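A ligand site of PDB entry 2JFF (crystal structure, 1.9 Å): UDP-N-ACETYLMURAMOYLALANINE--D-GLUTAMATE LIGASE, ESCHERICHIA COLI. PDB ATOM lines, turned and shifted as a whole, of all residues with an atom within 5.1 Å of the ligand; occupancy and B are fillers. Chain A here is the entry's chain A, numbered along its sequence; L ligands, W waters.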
ATOM      1  N   ILE A  12     -16.888  -9.937  -7.904  1.00  0.00           N
ATOM      2  CA  ILE A  12     -16.446 -11.024  -8.777  1.00  0.00           C
ATOM      3  C   ILE A  12     -17.579 -11.357  -9.726  1.00  0.00           C
ATOM      4  O   ILE A  12     -18.680 -11.734  -9.270  1.00  0.00           O
ATOM      5  CB  ILE A  12     -16.132 -12.285  -7.972  1.00  0.00           C
ATOM      6  CG1 ILE A  12     -15.135 -11.972  -6.822  1.00  0.00           C
ATOM      7  CG2 ILE A  12     -15.614 -13.382  -8.910  1.00  0.00           C
ATOM      8  CD1 ILE A  12     -14.854 -13.192  -5.905  1.00  0.00           C
ATOM      9  N   GLY A  13     -17.327 -11.213 -11.026  1.00  0.00           N
ATOM     10  CA  GLY A  13     -18.309 -11.531 -12.059  1.00  0.00           C
ATOM     11  C   GLY A  13     -18.927 -10.273 -12.613  1.00  0.00           C
ATOM     12  O   GLY A  13     -19.524  -9.460 -11.875  1.00  0.00           O
ATOM     13  N   ASP A  36     -13.090 -11.185 -12.943  1.00  0.00           N
ATOM     14  CA  ASP A  36     -13.910 -12.244 -13.556  1.00  0.00           C
ATOM     15  C   ASP A  36     -12.921 -13.287 -14.057  1.00  0.00           C
ATOM     16  O   ASP A  36     -11.865 -12.942 -14.590  1.00  0.00           O
ATOM     17  CB  ASP A  36     -14.777 -11.648 -14.694  1.00  0.00           C
ATOM     18  CG  ASP A  36     -15.948 -12.541 -15.115  1.00  0.00           C
ATOM     19  OD1 ASP A  36     -15.748 -13.726 -15.459  1.00  0.00           O
ATOM     20  OD2 ASP A  36     -17.083 -12.038 -15.127  1.00  0.00           O
ATOM     21  N   THR A  37     -13.244 -14.554 -13.852  1.00  0.00           N
ATOM     22  CA  THR A  37     -12.389 -15.642 -14.320  1.00  0.00           C
ATOM     23  C   THR A  37     -12.393 -15.783 -15.861  1.00  0.00           C
ATOM     24  O   THR A  37     -11.512 -16.421 -16.408  1.00  0.00           O
ATOM     25  CB  THR A  37     -12.797 -16.978 -13.684  1.00  0.00           C
ATOM     26  OG1 THR A  37     -14.203 -17.151 -13.858  1.00  0.00           O
ATOM     27  CG2 THR A  37     -12.453 -17.012 -12.204  1.00  0.00           C
ATOM     28  N   ARG A  38     -13.385 -15.196 -16.527  1.00  0.00           N
ATOM     29  CA  ARG A  38     -13.494 -15.231 -18.009  1.00  0.00           C
ATOM     30  C   ARG A  38     -12.670 -14.088 -18.621  1.00  0.00           C
ATOM     31  O   ARG A  38     -12.643 -12.996 -18.060  1.00  0.00           O
ATOM     32  CB  ARG A  38     -14.975 -15.116 -18.426  1.00  0.00           C
ATOM     33  CG  ARG A  38     -15.871 -16.176 -17.764  1.00  0.00           C
ATOM     34  CD  ARG A  38     -17.366 -15.838 -17.903  1.00  0.00           C
ATOM     35  NE  ARG A  38     -17.796 -14.697 -17.074  1.00  0.00           N
ATOM     36  CZ  ARG A  38     -19.061 -14.268 -16.993  1.00  0.00           C
ATOM     37  NH1 ARG A  38     -20.028 -14.878 -17.696  1.00  0.00           N
ATOM     38  NH2 ARG A  38     -19.357 -13.223 -16.246  1.00  0.00           N
ATOM     39  N   SER A  72     -20.514 -13.043  -7.551  1.00  0.00           N
ATOM     40  CA  SER A  72     -21.489 -13.617  -8.494  1.00  0.00           C
ATOM     41  C   SER A  72     -21.985 -14.979  -8.019  1.00  0.00           C
ATOM     42  O   SER A  72     -21.200 -15.772  -7.487  1.00  0.00           O
ATOM     43  CB  SER A  72     -20.845 -13.837  -9.855  1.00  0.00           C
ATOM     44  OG  SER A  72     -21.759 -14.568 -10.680  1.00  0.00           O
ATOM     45  N   PRO A  73     -23.289 -15.295  -8.245  1.00  0.00           N
ATOM     46  CA  PRO A  73     -23.739 -16.660  -7.983  1.00  0.00           C
ATOM     47  C   PRO A  73     -22.940 -17.694  -8.808  1.00  0.00           C
ATOM     48  O   PRO A  73     -22.899 -18.855  -8.447  1.00  0.00           O
ATOM     49  CB  PRO A  73     -25.217 -16.649  -8.426  1.00  0.00           C
ATOM     50  CG  PRO A  73     -25.367 -15.463  -9.295  1.00  0.00           C
ATOM     51  CD  PRO A  73     -24.391 -14.451  -8.752  1.00  0.00           C
ATOM     52  N   GLY A  74     -22.335 -17.255  -9.903  1.00  0.00           N
ATOM     53  CA  GLY A  74     -21.618 -18.128 -10.808  1.00  0.00           C
ATOM     54  C   GLY A  74     -20.239 -18.560 -10.302  1.00  0.00           C
ATOM     55  O   GLY A  74     -19.589 -19.368 -10.957  1.00  0.00           O
ATOM     56  N   ILE A  75     -19.794 -18.050  -9.154  1.00  0.00           N
ATOM     57  CA  ILE A  75     -18.543 -18.551  -8.592  1.00  0.00           C
ATOM     58  C   ILE A  75     -18.821 -19.298  -7.289  1.00  0.00           C
ATOM     59  O   ILE A  75     -19.538 -18.812  -6.421  1.00  0.00           O
ATOM     60  CB  ILE A  75     -17.450 -17.445  -8.416  1.00  0.00           C
ATOM     61  CG1 ILE A  75     -16.131 -18.120  -7.963  1.00  0.00           C
ATOM     62  CG2 ILE A  75     -17.856 -16.342  -7.399  1.00  0.00           C
ATOM     63  CD1 ILE A  75     -14.891 -17.420  -8.373  1.00  0.00           C
ATOM     64  N   ASN A 139     -33.184 -13.747 -10.330  1.00  0.00           N
ATOM     65  CA  ASN A 139     -32.499 -14.729 -11.151  1.00  0.00           C
ATOM     66  C   ASN A 139     -33.049 -14.788 -12.586  1.00  0.00           C
ATOM     67  O   ASN A 139     -32.416 -15.372 -13.480  1.00  0.00           O
ATOM     68  CB  ASN A 139     -32.559 -16.115 -10.512  1.00  0.00           C
ATOM     69  CG  ASN A 139     -31.605 -17.108 -11.165  1.00  0.00           C
ATOM     70  OD1 ASN A 139     -30.403 -16.822 -11.309  1.00  0.00           O
ATOM     71  ND2 ASN A 139     -32.129 -18.259 -11.577  1.00  0.00           N
ATOM     72  N   SER A 160     -31.914 -18.297  -7.180  1.00  0.00           N
ATOM     73  CA  SER A 160     -31.244 -19.588  -7.368  1.00  0.00           C
ATOM     74  C   SER A 160     -30.620 -20.123  -6.066  1.00  0.00           C
ATOM     75  O   SER A 160     -30.359 -19.352  -5.117  1.00  0.00           O
ATOM     76  CB  SER A 160     -30.161 -19.470  -8.450  1.00  0.00           C
ATOM     77  OG  SER A 160     -29.055 -18.697  -7.983  1.00  0.00           O
ATOM     78  N   PHE A 162     -27.579 -20.819  -5.802  1.00  0.00           N
ATOM     79  CA  PHE A 162     -26.302 -20.085  -5.721  1.00  0.00           C
ATOM     80  C   PHE A 162     -26.446 -18.722  -5.056  1.00  0.00           C
ATOM     81  O   PHE A 162     -25.671 -18.363  -4.165  1.00  0.00           O
ATOM     82  CB  PHE A 162     -25.668 -19.903  -7.090  1.00  0.00           C
ATOM     83  CG  PHE A 162     -25.370 -21.194  -7.827  1.00  0.00           C
ATOM     84  CD1 PHE A 162     -25.162 -22.402  -7.142  1.00  0.00           C
ATOM     85  CD2 PHE A 162     -25.224 -21.164  -9.218  1.00  0.00           C
ATOM     86  CE1 PHE A 162     -24.915 -23.604  -7.857  1.00  0.00           C
ATOM     87  CE2 PHE A 162     -24.910 -22.342  -9.941  1.00  0.00           C
ATOM     88  CZ  PHE A 162     -24.772 -23.560  -9.251  1.00  0.00           C
ATOM     89  N   ASP A 183     -29.711 -31.081  -9.665  1.00  0.00           N
ATOM     90  CA  ASP A 183     -29.198 -30.067 -10.594  1.00  0.00           C
ATOM     91  C   ASP A 183     -27.974 -29.444  -9.949  1.00  0.00           C
ATOM     92  O   ASP A 183     -27.764 -29.618  -8.755  1.00  0.00           O
ATOM     93  CB  ASP A 183     -30.304 -29.024 -10.870  1.00  0.00           C
ATOM     94  CG  ASP A 183     -29.986 -28.097 -12.045  1.00  0.00           C
ATOM     95  OD1 ASP A 183     -28.993 -28.280 -12.803  1.00  0.00           O
ATOM     96  OD2 ASP A 183     -30.780 -27.160 -12.228  1.00  0.00           O
ATOM     97  N   HIS A 184     -27.159 -28.760 -10.757  1.00  0.00           N
ATOM     98  CA  HIS A 184     -25.982 -28.016 -10.275  1.00  0.00           C
ATOM     99  C   HIS A 184     -24.973 -28.899  -9.540  1.00  0.00           C
ATOM    100  O   HIS A 184     -24.228 -28.418  -8.703  1.00  0.00           O
ATOM    101  CB  HIS A 184     -26.437 -26.835  -9.375  1.00  0.00           C
ATOM    102  CG  HIS A 184     -27.425 -25.918 -10.055  1.00  0.00           C
ATOM    103  ND1 HIS A 184     -27.143 -25.292 -11.244  1.00  0.00           N
ATOM    104  CD2 HIS A 184     -28.681 -25.535  -9.714  1.00  0.00           C
ATOM    105  CE1 HIS A 184     -28.177 -24.552 -11.607  1.00  0.00           C
ATOM    106  NE2 HIS A 184     -29.120 -24.669 -10.685  1.00  0.00           N
ATOM    107  N   THR A 322     -33.138 -27.077 -18.358  1.00  0.00           N
ATOM    108  CA  THR A 322     -31.682 -27.185 -18.160  1.00  0.00           C
ATOM    109  C   THR A 322     -31.300 -28.269 -17.145  1.00  0.00           C
ATOM    110  O   THR A 322     -30.142 -28.366 -16.709  1.00  0.00           O
ATOM    111  CB  THR A 322     -31.108 -25.832 -17.695  1.00  0.00           C
ATOM    112  OG1 THR A 322     -31.927 -25.338 -16.616  1.00  0.00           O
ATOM    113  CG2 THR A 322     -31.135 -24.818 -18.851  1.00  0.00           C
ATOM    114  N   LYS A 349     -23.908 -31.068 -16.332  1.00  0.00           N
ATOM    115  CA  LYS A 349     -23.544 -30.773 -14.918  1.00  0.00           C
ATOM    116  C   LYS A 349     -23.449 -32.033 -14.040  1.00  0.00           C
ATOM    117  O   LYS A 349     -23.870 -32.025 -12.879  1.00  0.00           O
ATOM    118  CB  LYS A 349     -24.518 -29.745 -14.311  1.00  0.00           C
ATOM    119  CG  LYS A 349     -24.452 -28.370 -15.000  1.00  0.00           C
ATOM    120  CD  LYS A 349     -25.708 -27.527 -14.695  1.00  0.00           C
ATOM    121  CE  LYS A 349     -26.905 -27.990 -15.578  1.00  0.00           C
ATOM    122  NZ  LYS A 349     -28.124 -27.184 -15.278  1.00  0.00           N
ATOM    123  N   CYS A 414     -30.062 -30.145 -19.990  1.00  0.00           N
ATOM    124  CA  CYS A 414     -28.682 -29.698 -19.781  1.00  0.00           C
ATOM    125  C   CYS A 414     -28.560 -28.201 -19.888  1.00  0.00           C
ATOM    126  O   CYS A 414     -29.367 -27.557 -20.570  1.00  0.00           O
ATOM    127  CB  CYS A 414     -27.739 -30.309 -20.836  1.00  0.00           C
ATOM    128  SG  CYS A 414     -27.675 -32.080 -20.915  1.00  0.00           S
ATOM    129  N   ALA A 415     -27.536 -27.651 -19.249  1.00  0.00           N
ATOM    130  CA  ALA A 415     -27.126 -26.277 -19.518  1.00  0.00           C
ATOM    131  C   ALA A 415     -26.601 -26.113 -20.963  1.00  0.00           C
ATOM    132  O   ALA A 415     -26.087 -27.063 -21.576  1.00  0.00           O
ATOM    133  CB  ALA A 415     -26.054 -25.831 -18.499  1.00  0.00           C
ATOM    134  N   SER A 416     -26.765 -24.916 -21.497  1.00  0.00           N
ATOM    135  CA  SER A 416     -26.367 -24.604 -22.866  1.00  0.00           C
ATOM    136  C   SER A 416     -24.961 -24.027 -22.925  1.00  0.00           C
ATOM    137  O   SER A 416     -24.403 -23.758 -24.014  1.00  0.00           O
ATOM    138  CB  SER A 416     -27.360 -23.590 -23.484  1.00  0.00           C
ATOM    139  OG  SER A 416     -27.236 -22.329 -22.839  1.00  0.00           O
ATOM    140  N   LEU A 417     -24.358 -23.814 -21.753  1.00  0.00           N
ATOM    141  CA  LEU A 417     -23.191 -22.946 -21.673  1.00  0.00           C
ATOM    142  C   LEU A 417     -21.932 -23.516 -22.350  1.00  0.00           C
ATOM    143  O   LEU A 417     -20.965 -22.775 -22.585  1.00  0.00           O
ATOM    144  CB  LEU A 417     -22.920 -22.538 -20.218  1.00  0.00           C
ATOM    145  CG  LEU A 417     -24.151 -21.989 -19.479  1.00  0.00           C
ATOM    146  CD1 LEU A 417     -23.809 -21.753 -17.972  1.00  0.00           C
ATOM    147  CD2 LEU A 417     -24.744 -20.725 -20.161  1.00  0.00           C
ATOM    148  N   ASN A 422     -26.494 -18.679 -23.368  1.00  0.00           N
ATOM    149  CA  ASN A 422     -27.555 -18.984 -22.398  1.00  0.00           C
ATOM    150  C   ASN A 422     -28.675 -19.770 -23.085  1.00  0.00           C
ATOM    151  O   ASN A 422     -28.663 -19.929 -24.293  1.00  0.00           O
ATOM    152  CB  ASN A 422     -28.107 -17.692 -21.761  1.00  0.00           C
ATOM    153  CG  ASN A 422     -28.447 -16.601 -22.796  1.00  0.00           C
ATOM    154  OD1 ASN A 422     -29.026 -16.859 -23.872  1.00  0.00           O
ATOM    155  ND2 ASN A 422     -28.088 -15.367 -22.471  1.00  0.00           N
ATOM    156  N   PHE A 423     -29.639 -20.293 -22.312  1.00  0.00           N
ATOM    157  CA  PHE A 423     -30.686 -21.129 -22.859  1.00  0.00           C
ATOM    158  C   PHE A 423     -31.565 -20.321 -23.829  1.00  0.00           C
ATOM    159  O   PHE A 423     -32.211 -20.911 -24.702  1.00  0.00           O
ATOM    160  CB  PHE A 423     -31.522 -21.746 -21.723  1.00  0.00           C
ATOM    161  CG  PHE A 423     -32.437 -20.759 -21.046  1.00  0.00           C
ATOM    162  CD1 PHE A 423     -33.697 -20.455 -21.598  1.00  0.00           C
ATOM    163  CD2 PHE A 423     -32.048 -20.143 -19.862  1.00  0.00           C
ATOM    164  CE1 PHE A 423     -34.558 -19.535 -20.977  1.00  0.00           C
ATOM    165  CE2 PHE A 423     -32.904 -19.206 -19.208  1.00  0.00           C
ATOM    166  CZ  PHE A 423     -34.157 -18.908 -19.764  1.00  0.00           C
ATOM    167  N   ARG A 426     -29.964 -20.523 -27.292  1.00  0.00           N
ATOM    168  CA  ARG A 426     -30.268 -21.881 -27.756  1.00  0.00           C
ATOM    169  C   ARG A 426     -31.720 -22.037 -28.261  1.00  0.00           C
ATOM    170  O   ARG A 426     -31.957 -22.586 -29.349  1.00  0.00           O
ATOM    171  CB  ARG A 426     -29.934 -22.921 -26.661  1.00  0.00           C
ATOM    172  CG  ARG A 426     -30.328 -24.349 -26.997  1.00  0.00           C
ATOM    173  CD  ARG A 426     -29.843 -25.300 -25.930  1.00  0.00           C
ATOM    174  NE  ARG A 426     -30.587 -25.140 -24.665  1.00  0.00           N
ATOM    175  CZ  ARG A 426     -30.257 -25.739 -23.526  1.00  0.00           C
ATOM    176  NH1 ARG A 426     -29.195 -26.533 -23.474  1.00  0.00           N
ATOM    177  NH2 ARG A 426     -30.997 -25.567 -22.435  1.00  0.00           N
HETATM  178  O1  LIG L   1     -26.483 -22.424 -12.792  1.00  0.00           O
HETATM  179  S1  LIG L   1     -26.708 -21.040 -13.201  1.00  0.00           S
HETATM  180  O2  LIG L   1     -27.488 -20.313 -12.172  1.00  0.00           O
HETATM  181  N1  LIG L   1     -27.616 -21.081 -14.544  1.00  0.00           N
HETATM  182  C1  LIG L   1     -27.379 -22.074 -15.595  1.00  0.00           C
HETATM  183  C2  LIG L   1     -27.921 -23.463 -15.263  1.00  0.00           C
HETATM  184  O3  LIG L   1     -28.970 -23.539 -14.602  1.00  0.00           O
HETATM  185  O4  LIG L   1     -27.302 -24.494 -15.655  1.00  0.00           O
HETATM  186  C3  LIG L   1     -27.996 -21.546 -16.900  1.00  0.00           C
HETATM  187  C4  LIG L   1     -27.973 -22.604 -18.026  1.00  0.00           C
HETATM  188  C5  LIG L   1     -28.343 -22.022 -19.369  1.00  0.00           C
HETATM  189  O5  LIG L   1     -28.243 -22.806 -20.333  1.00  0.00           O
HETATM  190  O6  LIG L   1     -28.729 -20.823 -19.487  1.00  0.00           O
HETATM  191  C6  LIG L   1     -25.300 -20.279 -13.530  1.00  0.00           C
HETATM  192  C7  LIG L   1     -24.216 -21.020 -14.022  1.00  0.00           C
HETATM  193  C8  LIG L   1     -22.998 -20.400 -14.329  1.00  0.00           C
HETATM  194  C9  LIG L   1     -22.843 -19.027 -14.126  1.00  0.00           C
HETATM  195  C10 LIG L   1     -23.930 -18.263 -13.627  1.00  0.00           C
HETATM  196  C11 LIG L   1     -25.154 -18.901 -13.353  1.00  0.00           C
HETATM  197  C12 LIG L   1     -21.614 -18.416 -14.423  1.00  0.00           C
HETATM  198  C13 LIG L   1     -21.469 -17.024 -14.220  1.00  0.00           C
HETATM  199  C14 LIG L   1     -22.537 -16.249 -13.733  1.00  0.00           C
HETATM  200  C15 LIG L   1     -23.776 -16.870 -13.434  1.00  0.00           C
HETATM  201  O7  LIG L   1     -20.245 -16.426 -14.504  1.00  0.00           O
HETATM  202  C16 LIG L   1     -19.019 -17.174 -14.487  1.00  0.00           C
HETATM  203  C17 LIG L   1     -17.888 -16.320 -13.933  1.00  0.00           C
HETATM  204  C18 LIG L   1     -18.044 -16.050 -12.446  1.00  0.00           C
HETATM  205  C19 LIG L   1     -16.853 -15.269 -11.952  1.00  0.00           C
HETATM  206  O   HOH W   1     -30.611 -25.615 -14.337  1.00  0.00           O
HETATM  207  O   HOH W   2     -28.951 -18.665 -15.185  1.00  0.00           O
HETATM  208  O   HOH W   3     -31.025 -21.534 -14.081  1.00  0.00           O
HETATM  209  O   HOH W   4     -30.400 -20.456 -11.791  1.00  0.00           O
HETATM  210  O   HOH W   5     -29.329 -18.893 -17.990  1.00  0.00           O
HETATM  211  O   HOH W   6     -27.869 -18.058 -10.136  1.00  0.00           O
HETATM  212  O   HOH W   7     -24.474 -24.318 -15.162  1.00  0.00           O
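Water W1 lies within hydrogen-bond range of the side-chain carboxylate of Asp 183, the side-chain hydroxyl of Thr 322, an oxygen (O3) of the ligand and the side-chain amino group of Lys 349. Water W4 lies within hydrogen-bond range of ND2 of Asn 139 (2.8 Å) and O2 of the ligand (2.9 Å). Water W6 lies within hydrogen-bond range of OG of Ser 160, OD1 of Asn 139 and O2 of the ligand.
A ring nitrogen (NE2) of His 184 is in hydrogen-bond range of the side-chain carboxylate (OD2) of Asp 183, 3.4 Å away. OG of Ser 416 sits at hydrogen-bond distance from N of Phe 423 (3.2 Å). The side-chain amino group of Lys 349 sits at hydrogen-bond distance from the backbone carbonyl oxygen of Thr 322 (2.7 Å). The side-chain amino group (NZ) of Lys 349 lies within salt-bridge range of the side-chain carboxylate (OD1) of Asp 183, 2.8 Å away. OG of Ser 72 lies within hydrogen-bond range of N of Gly 74 (2.9 Å). The backbone NH (N) of Phe 162 sits close to the side-chain hydroxyl (OG) of Ser 160, at 3.4 Å. The backbone carbonyl oxygen (O) of Ile 12 is in hydrogen-bond range of the backbone NH (N) of Ser 72 (2.8 Å). OD1 of Asp 36 lies within salt-bridge range of NE of Arg 38 (2.8 Å).
The backbone NH (N) of Ser 416 sits at hydrogen-bond distance from an oxygen (O5) of the ligand. O6 of the ligand sits at hydrogen-bond distance from N of Phe 423, 3.0 Å away. NZ of Lys 349 is in salt-bridge range of O4 of the ligand (2.8 Å). O5 of the ligand lies within hydrogen-bond range of OG of Ser 416. A ring nitrogen (ND1) of His 184 lies close to an oxygen (O1) of the ligand.
Residues that only touch the ligand: Ile 12, Asp 36, Thr 37, Arg 38, Ser 72, Gly 74, Phe 162, Thr 322, Ala 415, Leu 417 and Asn 422. Within 4 Å of the ligand: Ile 12, Asp 36, Thr 37, Arg 38, Ser 72, Gly 74, Phe 162, His 184, Thr 322, Lys 349, Ala 415, Ser 416, Leu 417, Asn 422 and Phe 423.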
